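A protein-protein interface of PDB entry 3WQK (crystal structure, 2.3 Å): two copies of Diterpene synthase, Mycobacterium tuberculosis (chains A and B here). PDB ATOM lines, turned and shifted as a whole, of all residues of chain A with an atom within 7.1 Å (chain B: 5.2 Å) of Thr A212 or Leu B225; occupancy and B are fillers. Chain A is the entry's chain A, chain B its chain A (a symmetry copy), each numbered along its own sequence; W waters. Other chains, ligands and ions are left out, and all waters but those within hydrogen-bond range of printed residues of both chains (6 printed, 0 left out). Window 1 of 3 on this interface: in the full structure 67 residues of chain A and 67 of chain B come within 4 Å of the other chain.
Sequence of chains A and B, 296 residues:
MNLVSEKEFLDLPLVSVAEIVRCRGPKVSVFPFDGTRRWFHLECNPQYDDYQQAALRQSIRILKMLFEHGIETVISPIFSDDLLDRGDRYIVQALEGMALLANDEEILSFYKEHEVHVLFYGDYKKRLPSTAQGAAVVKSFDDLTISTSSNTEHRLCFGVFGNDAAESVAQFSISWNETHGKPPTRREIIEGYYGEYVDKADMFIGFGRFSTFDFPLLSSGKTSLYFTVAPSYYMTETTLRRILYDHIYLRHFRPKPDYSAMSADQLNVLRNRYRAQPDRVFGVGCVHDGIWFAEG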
ATOM      1  N   PHE A 204      13.232   3.986  37.271  1.00  0.00           N
ATOM      2  CA  PHE A 204      11.795   4.135  37.207  1.00  0.00           C
ATOM      3  C   PHE A 204      11.246   2.801  36.752  1.00  0.00           C
ATOM      4  O   PHE A 204      11.651   2.275  35.705  1.00  0.00           O
ATOM      5  CB  PHE A 204      11.408   5.227  36.206  1.00  0.00           C
ATOM      6  CG  PHE A 204       9.919   5.400  36.030  1.00  0.00           C
ATOM      7  CD1 PHE A 204       9.174   4.484  35.284  1.00  0.00           C
ATOM      8  CD2 PHE A 204       9.264   6.498  36.592  1.00  0.00           C
ATOM      9  CE1 PHE A 204       7.791   4.659  35.095  1.00  0.00           C
ATOM     10  CE2 PHE A 204       7.889   6.683  36.411  1.00  0.00           C
ATOM     11  CZ  PHE A 204       7.149   5.757  35.658  1.00  0.00           C
ATOM     12  N   GLY A 206       7.931   1.174  35.578  1.00  0.00           N
ATOM     13  CA  GLY A 206       6.550   1.343  35.184  1.00  0.00           C
ATOM     14  C   GLY A 206       6.022  -0.001  34.731  1.00  0.00           C
ATOM     15  O   GLY A 206       6.564  -1.041  35.105  1.00  0.00           O
ATOM     16  N   ARG A 209       2.626   0.170  28.564  1.00  0.00           N
ATOM     17  CA  ARG A 209       3.129   1.176  27.632  1.00  0.00           C
ATOM     18  C   ARG A 209       4.403   1.854  28.151  1.00  0.00           C
ATOM     19  O   ARG A 209       4.451   2.304  29.295  1.00  0.00           O
ATOM     20  CB  ARG A 209       2.037   2.227  27.370  1.00  0.00           C
ATOM     21  CG  ARG A 209       0.956   1.743  26.396  1.00  0.00           C
ATOM     22  CD  ARG A 209      -0.245   2.682  26.369  1.00  0.00           C
ATOM     23  NE  ARG A 209      -0.822   2.808  27.703  1.00  0.00           N
ATOM     24  CZ  ARG A 209      -1.869   3.570  27.997  1.00  0.00           C
ATOM     25  NH1 ARG A 209      -2.463   4.275  27.039  1.00  0.00           N
ATOM     26  NH2 ARG A 209      -2.308   3.646  29.249  1.00  0.00           N
ATOM     27  N   PHE A 210       5.429   1.914  27.306  1.00  0.00           N
ATOM     28  CA  PHE A 210       6.706   2.522  27.681  1.00  0.00           C
ATOM     29  C   PHE A 210       6.525   4.036  27.829  1.00  0.00           C
ATOM     30  O   PHE A 210       6.460   4.765  26.836  1.00  0.00           O
ATOM     31  CB  PHE A 210       7.786   2.255  26.610  1.00  0.00           C
ATOM     32  CG  PHE A 210       8.260   0.814  26.525  1.00  0.00           C
ATOM     33  CD1 PHE A 210       7.544  -0.230  27.117  1.00  0.00           C
ATOM     34  CD2 PHE A 210       9.431   0.503  25.817  1.00  0.00           C
ATOM     35  CE1 PHE A 210       7.981  -1.559  27.008  1.00  0.00           C
ATOM     36  CE2 PHE A 210       9.877  -0.820  25.703  1.00  0.00           C
ATOM     37  CZ  PHE A 210       9.152  -1.854  26.299  1.00  0.00           C
ATOM     38  N   SER A 211       6.463   4.505  29.067  1.00  0.00           N
ATOM     39  CA  SER A 211       6.294   5.928  29.330  1.00  0.00           C
ATOM     40  C   SER A 211       6.585   6.196  30.795  1.00  0.00           C
ATOM     41  O   SER A 211       6.407   5.315  31.643  1.00  0.00           O
ATOM     42  CB  SER A 211       4.862   6.378  29.009  1.00  0.00           C
ATOM     43  OG  SER A 211       4.019   6.287  30.142  1.00  0.00           O
ATOM     44  N   THR A 212       7.039   7.411  31.083  1.00  0.00           N
ATOM     45  CA  THR A 212       7.358   7.794  32.444  1.00  0.00           C
ATOM     46  C   THR A 212       6.562   9.045  32.776  1.00  0.00           C
ATOM     47  O   THR A 212       6.135   9.770  31.884  1.00  0.00           O
ATOM     48  CB  THR A 212       8.863   8.094  32.598  1.00  0.00           C
ATOM     49  OG1 THR A 212       9.182   9.300  31.894  1.00  0.00           O
ATOM     50  CG2 THR A 212       9.692   6.946  32.019  1.00  0.00           C
ATOM     51  N   PHE A 213       6.378   9.313  34.058  1.00  0.00           N
ATOM     52  CA  PHE A 213       5.592  10.469  34.442  1.00  0.00           C
ATOM     53  C   PHE A 213       5.661  10.785  35.916  1.00  0.00           C
ATOM     54  O   PHE A 213       5.965   9.921  36.742  1.00  0.00           O
ATOM     55  CB  PHE A 213       4.112  10.225  34.092  1.00  0.00           C
ATOM     56  CG  PHE A 213       3.606   8.880  34.549  1.00  0.00           C
ATOM     57  CD1 PHE A 213       3.765   7.750  33.749  1.00  0.00           C
ATOM     58  CD2 PHE A 213       3.038   8.725  35.813  1.00  0.00           C
ATOM     59  CE1 PHE A 213       3.369   6.479  34.205  1.00  0.00           C
ATOM     60  CE2 PHE A 213       2.638   7.465  36.277  1.00  0.00           C
ATOM     61  CZ  PHE A 213       2.807   6.339  35.470  1.00  0.00           C
ATOM     62  N   ASP A 214       5.388  12.050  36.223  1.00  0.00           N
ATOM     63  CA  ASP A 214       5.282  12.512  37.594  1.00  0.00           C
ATOM     64  C   ASP A 214       6.459  12.482  38.572  1.00  0.00           C
ATOM     65  O   ASP A 214       6.275  12.154  39.740  1.00  0.00           O
ATOM     66  CB  ASP A 214       4.081  11.812  38.244  1.00  0.00           C
ATOM     67  CG  ASP A 214       2.740  12.224  37.618  1.00  0.00           C
ATOM     68  OD1 ASP A 214       2.712  12.747  36.484  1.00  0.00           O
ATOM     69  OD2 ASP A 214       1.694  12.012  38.269  1.00  0.00           O
ATOM     70  N   PHE A 215       7.665  12.790  38.115  1.00  0.00           N
ATOM     71  CA  PHE A 215       8.772  12.903  39.058  1.00  0.00           C
ATOM     72  C   PHE A 215       9.607  14.074  38.563  1.00  0.00           C
ATOM     73  O   PHE A 215      10.777  13.951  38.223  1.00  0.00           O
ATOM     74  CB  PHE A 215       9.570  11.584  39.251  1.00  0.00           C
ATOM     75  CG  PHE A 215      10.185  11.005  38.005  1.00  0.00           C
ATOM     76  CD1 PHE A 215       9.393  10.447  37.003  1.00  0.00           C
ATOM     77  CD2 PHE A 215      11.570  10.943  37.874  1.00  0.00           C
ATOM     78  CE1 PHE A 215       9.978   9.832  35.891  1.00  0.00           C
ATOM     79  CE2 PHE A 215      12.159  10.335  36.775  1.00  0.00           C
ATOM     80  CZ  PHE A 215      11.366   9.775  35.778  1.00  0.00           C
ATOM     81  N   SER A 219      14.598  13.621  37.065  1.00  0.00           N
ATOM     82  CA  SER A 219      14.970  12.762  35.958  1.00  0.00           C
ATOM     83  C   SER A 219      16.270  13.152  35.275  1.00  0.00           C
ATOM     84  O   SER A 219      16.564  14.335  35.105  1.00  0.00           O
ATOM     85  CB  SER A 219      13.845  12.737  34.917  1.00  0.00           C
ATOM     86  OG  SER A 219      14.238  12.016  33.758  1.00  0.00           O
ATOM     87  N   THR A 223      18.624   7.819  34.932  1.00  0.00           N
ATOM     88  CA  THR A 223      17.465   7.162  35.531  1.00  0.00           C
ATOM     89  C   THR A 223      17.164   5.917  34.682  1.00  0.00           C
ATOM     90  O   THR A 223      16.629   6.029  33.583  1.00  0.00           O
ATOM     91  CB  THR A 223      16.221   8.088  35.536  1.00  0.00           C
ATOM     92  OG1 THR A 223      16.508   9.262  36.303  1.00  0.00           O
ATOM     93  CG2 THR A 223      15.016   7.373  36.146  1.00  0.00           C
ATOM     94  N   LEU A 225      15.331   2.953  33.129  1.00  0.00           N
ATOM     95  CA  LEU A 225      13.907   2.662  32.946  1.00  0.00           C
ATOM     96  C   LEU A 225      13.572   1.187  32.749  1.00  0.00           C
ATOM     97  O   LEU A 225      14.261   0.471  32.016  1.00  0.00           O
ATOM     98  CB  LEU A 225      13.352   3.470  31.770  1.00  0.00           C
ATOM     99  CG  LEU A 225      13.686   4.967  31.838  1.00  0.00           C
ATOM    100  CD1 LEU A 225      13.086   5.678  30.620  1.00  0.00           C
ATOM    101  CD2 LEU A 225      13.154   5.570  33.168  1.00  0.00           C
ATOM    102  N   TYR A 226      12.513   0.749  33.429  1.00  0.00           N
ATOM    103  CA  TYR A 226      12.011  -0.621  33.341  1.00  0.00           C
ATOM    104  C   TYR A 226      10.487  -0.593  33.233  1.00  0.00           C
ATOM    105  O   TYR A 226       9.815   0.245  33.861  1.00  0.00           O
ATOM    106  CB  TYR A 226      12.392  -1.422  34.583  1.00  0.00           C
ATOM    107  CG  TYR A 226      13.874  -1.427  34.836  1.00  0.00           C
ATOM    108  CD1 TYR A 226      14.710  -2.335  34.194  1.00  0.00           C
ATOM    109  CD2 TYR A 226      14.449  -0.473  35.671  1.00  0.00           C
ATOM    110  CE1 TYR A 226      16.091  -2.290  34.379  1.00  0.00           C
ATOM    111  CE2 TYR A 226      15.810  -0.413  35.859  1.00  0.00           C
ATOM    112  CZ  TYR A 226      16.627  -1.318  35.215  1.00  0.00           C
ATOM    113  OH  TYR A 226      17.969  -1.218  35.401  1.00  0.00           O
ATOM    114  N   PHE A 227       9.948  -1.533  32.459  1.00  0.00           N
ATOM    115  CA  PHE A 227       8.516  -1.647  32.254  1.00  0.00           C
ATOM    116  C   PHE A 227       8.105  -3.111  32.332  1.00  0.00           C
ATOM    117  O   PHE A 227       8.380  -3.890  31.421  1.00  0.00           O
ATOM    118  CB  PHE A 227       8.137  -1.085  30.880  1.00  0.00           C
ATOM    119  CG  PHE A 227       8.611   0.316  30.660  1.00  0.00           C
ATOM    120  CD1 PHE A 227       7.996   1.385  31.315  1.00  0.00           C
ATOM    121  CD2 PHE A 227       9.710   0.568  29.854  1.00  0.00           C
ATOM    122  CE1 PHE A 227       8.477   2.684  31.169  1.00  0.00           C
ATOM    123  CE2 PHE A 227      10.200   1.860  29.704  1.00  0.00           C
ATOM    124  CZ  PHE A 227       9.579   2.921  30.365  1.00  0.00           C
ATOM    125  N   VAL A 281      13.177  -2.683  17.378  1.00  0.00           N
ATOM    126  CA  VAL A 281      12.901  -1.577  18.288  1.00  0.00           C
ATOM    127  C   VAL A 281      11.978  -2.003  19.418  1.00  0.00           C
ATOM    128  O   VAL A 281      10.998  -2.698  19.185  1.00  0.00           O
ATOM    129  CB  VAL A 281      12.244  -0.395  17.537  1.00  0.00           C
ATOM    130  CG1 VAL A 281      11.152  -0.911  16.619  1.00  0.00           C
ATOM    131  CG2 VAL A 281      11.671   0.623  18.537  1.00  0.00           C
ATOM    132  N   PHE A 282      12.302  -1.592  20.643  1.00  0.00           N
ATOM    133  CA  PHE A 282      11.482  -1.902  21.806  1.00  0.00           C
ATOM    134  C   PHE A 282      10.560  -0.716  22.060  1.00  0.00           C
ATOM    135  O   PHE A 282      10.996   0.448  22.015  1.00  0.00           O
ATOM    136  CB  PHE A 282      12.362  -2.157  23.030  1.00  0.00           C
ATOM    137  CG  PHE A 282      13.121  -3.453  22.962  1.00  0.00           C
ATOM    138  CD1 PHE A 282      12.491  -4.660  23.255  1.00  0.00           C
ATOM    139  CD2 PHE A 282      14.444  -3.474  22.543  1.00  0.00           C
ATOM    140  CE1 PHE A 282      13.171  -5.874  23.126  1.00  0.00           C
ATOM    141  CE2 PHE A 282      15.133  -4.679  22.409  1.00  0.00           C
ATOM    142  CZ  PHE A 282      14.496  -5.886  22.699  1.00  0.00           C
ATOM    143  N   GLY A 283       9.288  -1.011  22.324  1.00  0.00           N
ATOM    144  CA  GLY A 283       8.316   0.045  22.558  1.00  0.00           C
ATOM    145  C   GLY A 283       7.103  -0.049  21.637  1.00  0.00           C
ATOM    146  O   GLY A 283       6.061   0.550  21.912  1.00  0.00           O
ATOM    147  N   VAL A 284       7.238  -0.765  20.523  1.00  0.00           N
ATOM    148  CA  VAL A 284       6.106  -0.947  19.619  1.00  0.00           C
ATOM    149  C   VAL A 284       5.326  -2.131  20.194  1.00  0.00           C
ATOM    150  O   VAL A 284       5.921  -3.109  20.667  1.00  0.00           O
ATOM    151  CB  VAL A 284       6.554  -1.271  18.166  1.00  0.00           C
ATOM    152  CG1 VAL A 284       7.265  -0.061  17.549  1.00  0.00           C
ATOM    153  CG2 VAL A 284       7.462  -2.476  18.163  1.00  0.00           C
ATOM    154  N   TRP A 292      -2.806  -2.422  25.499  1.00  0.00           N
ATOM    155  CA  TRP A 292      -1.547  -2.445  24.775  1.00  0.00           C
ATOM    156  C   TRP A 292      -0.534  -3.379  25.449  1.00  0.00           C
ATOM    157  O   TRP A 292      -0.407  -3.385  26.673  1.00  0.00           O
ATOM    158  CB  TRP A 292      -0.994  -1.014  24.729  1.00  0.00           C
ATOM    159  CG  TRP A 292       0.261  -0.832  23.943  1.00  0.00           C
ATOM    160  CD1 TRP A 292       0.364  -0.391  22.659  1.00  0.00           C
ATOM    161  CD2 TRP A 292       1.599  -1.054  24.402  1.00  0.00           C
ATOM    162  NE1 TRP A 292       1.689  -0.321  22.283  1.00  0.00           N
ATOM    163  CE2 TRP A 292       2.467  -0.722  23.338  1.00  0.00           C
ATOM    164  CE3 TRP A 292       2.151  -1.502  25.614  1.00  0.00           C
ATOM    165  CZ2 TRP A 292       3.862  -0.821  23.447  1.00  0.00           C
ATOM    166  CZ3 TRP A 292       3.529  -1.602  25.723  1.00  0.00           C
ATOM    167  CH2 TRP A 292       4.369  -1.262  24.645  1.00  0.00           C
ATOM    168  N   PHE B 204       9.528   9.868  22.200  1.00  0.00           N
ATOM    169  CA  PHE B 204      10.964   9.947  22.354  1.00  0.00           C
ATOM    170  C   PHE B 204      11.527   8.663  21.784  1.00  0.00           C
ATOM    171  O   PHE B 204      11.131   7.563  22.194  1.00  0.00           O
ATOM    172  CB  PHE B 204      11.345  10.073  23.831  1.00  0.00           C
ATOM    173  CG  PHE B 204      12.832  10.094  24.084  1.00  0.00           C
ATOM    174  CD1 PHE B 204      13.588   8.921  24.012  1.00  0.00           C
ATOM    175  CD2 PHE B 204      13.475  11.287  24.419  1.00  0.00           C
ATOM    176  CE1 PHE B 204      14.971   8.935  24.274  1.00  0.00           C
ATOM    177  CE2 PHE B 204      14.849  11.313  24.682  1.00  0.00           C
ATOM    178  CZ  PHE B 204      15.600  10.129  24.609  1.00  0.00           C
ATOM    179  N   THR B 212      15.711   8.237  29.091  1.00  0.00           N
ATOM    180  CA  THR B 212      15.384   9.440  28.351  1.00  0.00           C
ATOM    181  C   THR B 212      16.168  10.590  28.959  1.00  0.00           C
ATOM    182  O   THR B 212      16.591  10.521  30.108  1.00  0.00           O
ATOM    183  CB  THR B 212      13.875   9.751  28.436  1.00  0.00           C
ATOM    184  OG1 THR B 212      13.548  10.155  29.770  1.00  0.00           O
ATOM    185  CG2 THR B 212      13.059   8.507  28.079  1.00  0.00           C
ATOM    186  N   SER B 219       8.074  16.788  28.890  1.00  0.00           N
ATOM    187  CA  SER B 219       7.714  15.402  29.118  1.00  0.00           C
ATOM    188  C   SER B 219       6.413  15.213  29.879  1.00  0.00           C
ATOM    189  O   SER B 219       6.109  15.963  30.806  1.00  0.00           O
ATOM    190  CB  SER B 219       8.842  14.687  29.869  1.00  0.00           C
ATOM    191  OG  SER B 219       8.460  13.368  30.228  1.00  0.00           O
ATOM    192  N   SER B 220       5.644  14.210  29.470  1.00  0.00           N
ATOM    193  CA  SER B 220       4.405  13.858  30.149  1.00  0.00           C
ATOM    194  C   SER B 220       4.203  12.352  29.996  1.00  0.00           C
ATOM    195  O   SER B 220       4.953  11.677  29.271  1.00  0.00           O
ATOM    196  CB  SER B 220       3.199  14.604  29.558  1.00  0.00           C
ATOM    197  OG  SER B 220       2.702  13.971  28.392  1.00  0.00           O
ATOM    198  N   GLY B 221       3.194  11.832  30.688  1.00  0.00           N
ATOM    199  CA  GLY B 221       2.882  10.417  30.594  1.00  0.00           C
ATOM    200  C   GLY B 221       2.452  10.066  29.177  1.00  0.00           C
ATOM    201  O   GLY B 221       2.408   8.888  28.800  1.00  0.00           O
ATOM    202  N   THR B 223       4.109  11.043  26.500  1.00  0.00           N
ATOM    203  CA  THR B 223       5.272  10.978  25.619  1.00  0.00           C
ATOM    204  C   THR B 223       5.588   9.491  25.398  1.00  0.00           C
ATOM    205  O   THR B 223       6.125   8.832  26.283  1.00  0.00           O
ATOM    206  CB  THR B 223       6.507  11.673  26.248  1.00  0.00           C
ATOM    207  OG1 THR B 223       6.207  13.054  26.482  1.00  0.00           O
ATOM    208  CG2 THR B 223       7.717  11.574  25.320  1.00  0.00           C
ATOM    209  N   SER B 224       5.235   8.972  24.227  1.00  0.00           N
ATOM    210  CA  SER B 224       5.469   7.561  23.894  1.00  0.00           C
ATOM    211  C   SER B 224       6.967   7.256  23.781  1.00  0.00           C
ATOM    212  O   SER B 224       7.675   7.896  23.005  1.00  0.00           O
ATOM    213  CB  SER B 224       4.781   7.224  22.566  1.00  0.00           C
ATOM    214  OG  SER B 224       3.373   7.410  22.634  1.00  0.00           O
ATOM    215  N   LEU B 225       7.453   6.278  24.532  1.00  0.00           N
ATOM    216  CA  LEU B 225       8.880   5.953  24.474  1.00  0.00           C
ATOM    217  C   LEU B 225       9.230   4.740  23.618  1.00  0.00           C
ATOM    218  O   LEU B 225       8.550   3.710  23.668  1.00  0.00           O
ATOM    219  CB  LEU B 225       9.433   5.753  25.887  1.00  0.00           C
ATOM    220  CG  LEU B 225       9.084   6.895  26.853  1.00  0.00           C
ATOM    221  CD1 LEU B 225       9.682   6.595  28.232  1.00  0.00           C
ATOM    222  CD2 LEU B 225       9.606   8.246  26.288  1.00  0.00           C
ATOM    223  N   TYR B 226      10.291   4.889  22.825  1.00  0.00           N
ATOM    224  CA  TYR B 226      10.806   3.829  21.962  1.00  0.00           C
ATOM    225  C   TYR B 226      12.330   3.790  22.065  1.00  0.00           C
ATOM    226  O   TYR B 226      12.991   4.838  22.176  1.00  0.00           O
ATOM    227  CB  TYR B 226      10.427   4.081  20.505  1.00  0.00           C
ATOM    228  CG  TYR B 226       8.944   4.235  20.310  1.00  0.00           C
ATOM    229  CD1 TYR B 226       8.120   3.125  20.162  1.00  0.00           C
ATOM    230  CD2 TYR B 226       8.358   5.497  20.343  1.00  0.00           C
ATOM    231  CE1 TYR B 226       6.738   3.271  20.051  1.00  0.00           C
ATOM    232  CE2 TYR B 226       6.995   5.656  20.240  1.00  0.00           C
ATOM    233  CZ  TYR B 226       6.189   4.547  20.096  1.00  0.00           C
ATOM    234  OH  TYR B 226       4.846   4.735  20.022  1.00  0.00           O
ATOM    235  N   PHE B 227      12.880   2.579  21.997  1.00  0.00           N
ATOM    236  CA  PHE B 227      14.314   2.370  22.075  1.00  0.00           C
ATOM    237  C   PHE B 227      14.738   1.351  21.025  1.00  0.00           C
ATOM    238  O   PHE B 227      14.473   0.159  21.164  1.00  0.00           O
ATOM    239  CB  PHE B 227      14.692   1.853  23.467  1.00  0.00           C
ATOM    240  CG  PHE B 227      14.206   2.727  24.578  1.00  0.00           C
ATOM    241  CD1 PHE B 227      14.810   3.962  24.826  1.00  0.00           C
ATOM    242  CD2 PHE B 227      13.108   2.355  25.337  1.00  0.00           C
ATOM    243  CE1 PHE B 227      14.317   4.812  25.813  1.00  0.00           C
ATOM    244  CE2 PHE B 227      12.607   3.196  26.323  1.00  0.00           C
ATOM    245  CZ  PHE B 227      13.215   4.430  26.560  1.00  0.00           C
ATOM    246  N   ARG B 251      -0.942   3.172  20.934  1.00  0.00           N
ATOM    247  CA  ARG B 251      -0.757   3.680  22.293  1.00  0.00           C
ATOM    248  C   ARG B 251      -2.062   4.110  22.943  1.00  0.00           C
ATOM    249  O   ARG B 251      -2.358   3.698  24.066  1.00  0.00           O
ATOM    250  CB  ARG B 251       0.270   4.829  22.330  1.00  0.00           C
ATOM    251  CG  ARG B 251       1.730   4.374  22.183  1.00  0.00           C
ATOM    252  CD  ARG B 251       2.109   3.266  23.203  1.00  0.00           C
ATOM    253  NE  ARG B 251       3.497   2.827  23.050  1.00  0.00           N
ATOM    254  CZ  ARG B 251       4.535   3.304  23.749  1.00  0.00           C
ATOM    255  NH1 ARG B 251       4.364   4.237  24.678  1.00  0.00           N
ATOM    256  NH2 ARG B 251       5.757   2.863  23.496  1.00  0.00           N
HETATM  257  O   HOH W   1      13.894  13.218  30.516  1.00  0.00           O
HETATM  258  O   HOH W   2       8.978  10.874  29.131  1.00  0.00           O
HETATM  259  O   HOH W   3       6.743   9.275  28.805  1.00  0.00           O
HETATM  260  O   HOH W   4      15.999   8.061  32.030  1.00  0.00           O
HETATM  261  O   HOH W   5      13.748   9.436  32.868  1.00  0.00           O
HETATM  262  O   HOH W   6       8.806  12.052  33.425  1.00  0.00           O
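Hydrophobic or aromatic side chains of chain A within 4 Å of the printed part of chain B: Phe A210, Phe A213, Leu A225, Val A281, Phe A282 and Trp A292. Of the 11 printed residues of chain B, 9 touch a printed residue of chain A. Along chain B the printed residues that touch a printed residue of chain A span positions 212 to 251. Among the printed residues, 19 pairs touch across the chains.
Water W4 lies within hydrogen-bond range of O of Thr A223 and N of Thr B212. Water W3 lies within hydrogen-bond range of O of Thr B223, N of Thr A212 and O of Ser B220. Water W5 bridges the side-chain hydroxyl (OG) of Ser A219 (2.8 Å) and the side-chain hydroxyl (OG1) of Thr B212 (3.2 Å). Water W2 lies within hydrogen-bond range of the side-chain hydroxyl of Ser B219 (2.8 Å) and the side-chain hydroxyl of Thr A212 (3.2 Å). Water W6 bridges the side-chain hydroxyl (OG1) of Thr A212 (3.2 Å) and the side-chain hydroxyl (OG) of Ser B219 (3.5 Å). Water W1 lies within hydrogen-bond range of OG1 of Thr B212 (3.2 Å) and OG of Ser A219 (3.5 Å).
Thr A212 touches Leu B225, and with the chains exchanged Leu A225 touches Thr B212. Of the 19 pairs that touch across the chains among the printed residues, 2 have their exchanged pair printed and touching as well.
Of the printed residues of chain B, Thr A212 touches Ser B220 (3.4 Å), Gly B221 (3.6 Å) and Leu B225 (3.8 Å). Leu B225 touches just these residues of chain A: Phe A210, Ser A211, Thr A212 and Gly A283. Printed residues of chain B within 4 Å of Phe A210: Ser B224 (3.97 Å), Leu B225 (2.9 Å) and Arg B251 (3.1 Å). Of the printed residues of chain A, Phe B227 touches Val A281 (3.7 Å) and Phe A282 (2.8 Å). Of the printed residues of chain A, Ser B220 touches Thr A212 (3.4 Å). Printed residues of chain B within 4 Å of Leu A225: Thr B212. Ser B219 touches none of the printed residues of chain A. Asp A214 touches none of the printed residues of chain B. The nearest residue of chain B that does not touch Thr A212 is Ser B219 (4.5 Å). The nearest printed residue of chain A that does not touch Leu B225 is Phe A227 (4.2 Å). The nearest printed residue of chain B that does not touch Phe A282 is Leu B225 (4.4 Å).
The backbone NH (N) of Phe B204 sits at hydrogen-bond distance from the backbone carbonyl oxygen (O) of Ser B224 (2.8 Å). N of Tyr B226 is in hydrogen-bond range of O of Phe B204. N of Ser B220 is in hydrogen-bond range of OG1 of Thr B223 (3.3 Å). The guanidinium group (NH2) of Arg B251 lies within hydrogen-bond range of the backbone carbonyl oxygen (O) of Leu B225.
The guanidinium group of Arg A209 is in hydrogen-bond range of the backbone carbonyl oxygen of Arg B251 (3.0 Å). The backbone carbonyl oxygen (O) of Phe A210 sits at hydrogen-bond distance from the backbone NH (N) of Leu B225 (2.9 Å). The backbone carbonyl oxygen of Phe A210 is in hydrogen-bond range of the guanidinium group of Arg B251, 3.1 Å away. The backbone carbonyl oxygen (O) of Gly B221 sits at hydrogen-bond distance from the side-chain hydroxyl (OG) of Ser A211. The backbone NH (N) of Phe A282 sits at hydrogen-bond distance from the backbone carbonyl oxygen (O) of Phe B227, 2.8 Å away. The backbone carbonyl oxygen (O) of Gly A283 sits at hydrogen-bond distance from the guanidinium group (NH2) of Arg B251 (2.8 Å). The backbone carbonyl oxygen (O) of Thr A212 sits close to the backbone carbonyl oxygen (O) of Ser B220 (3.4 Å).
Leu B225 touches Ser A211 (CD1 to CA, 3.6 Å). O of Thr A212 touches CA of Gly B221, 3.6 Å away. Leu B225 touches Thr A212. Phe A213 touches Gly B221. Leu A225 touches Thr B212 (CD1 to CG2, 3.8 Å). Phe B227 touches Val A281. Phe A282 touches Tyr B226. Leu B225 touches Gly A283. Tyr B226 touches Gly A283 (CE1 to O, 3.4 Å). CZ2 of Trp A292 touches NE of Arg B251 (3.7 Å).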
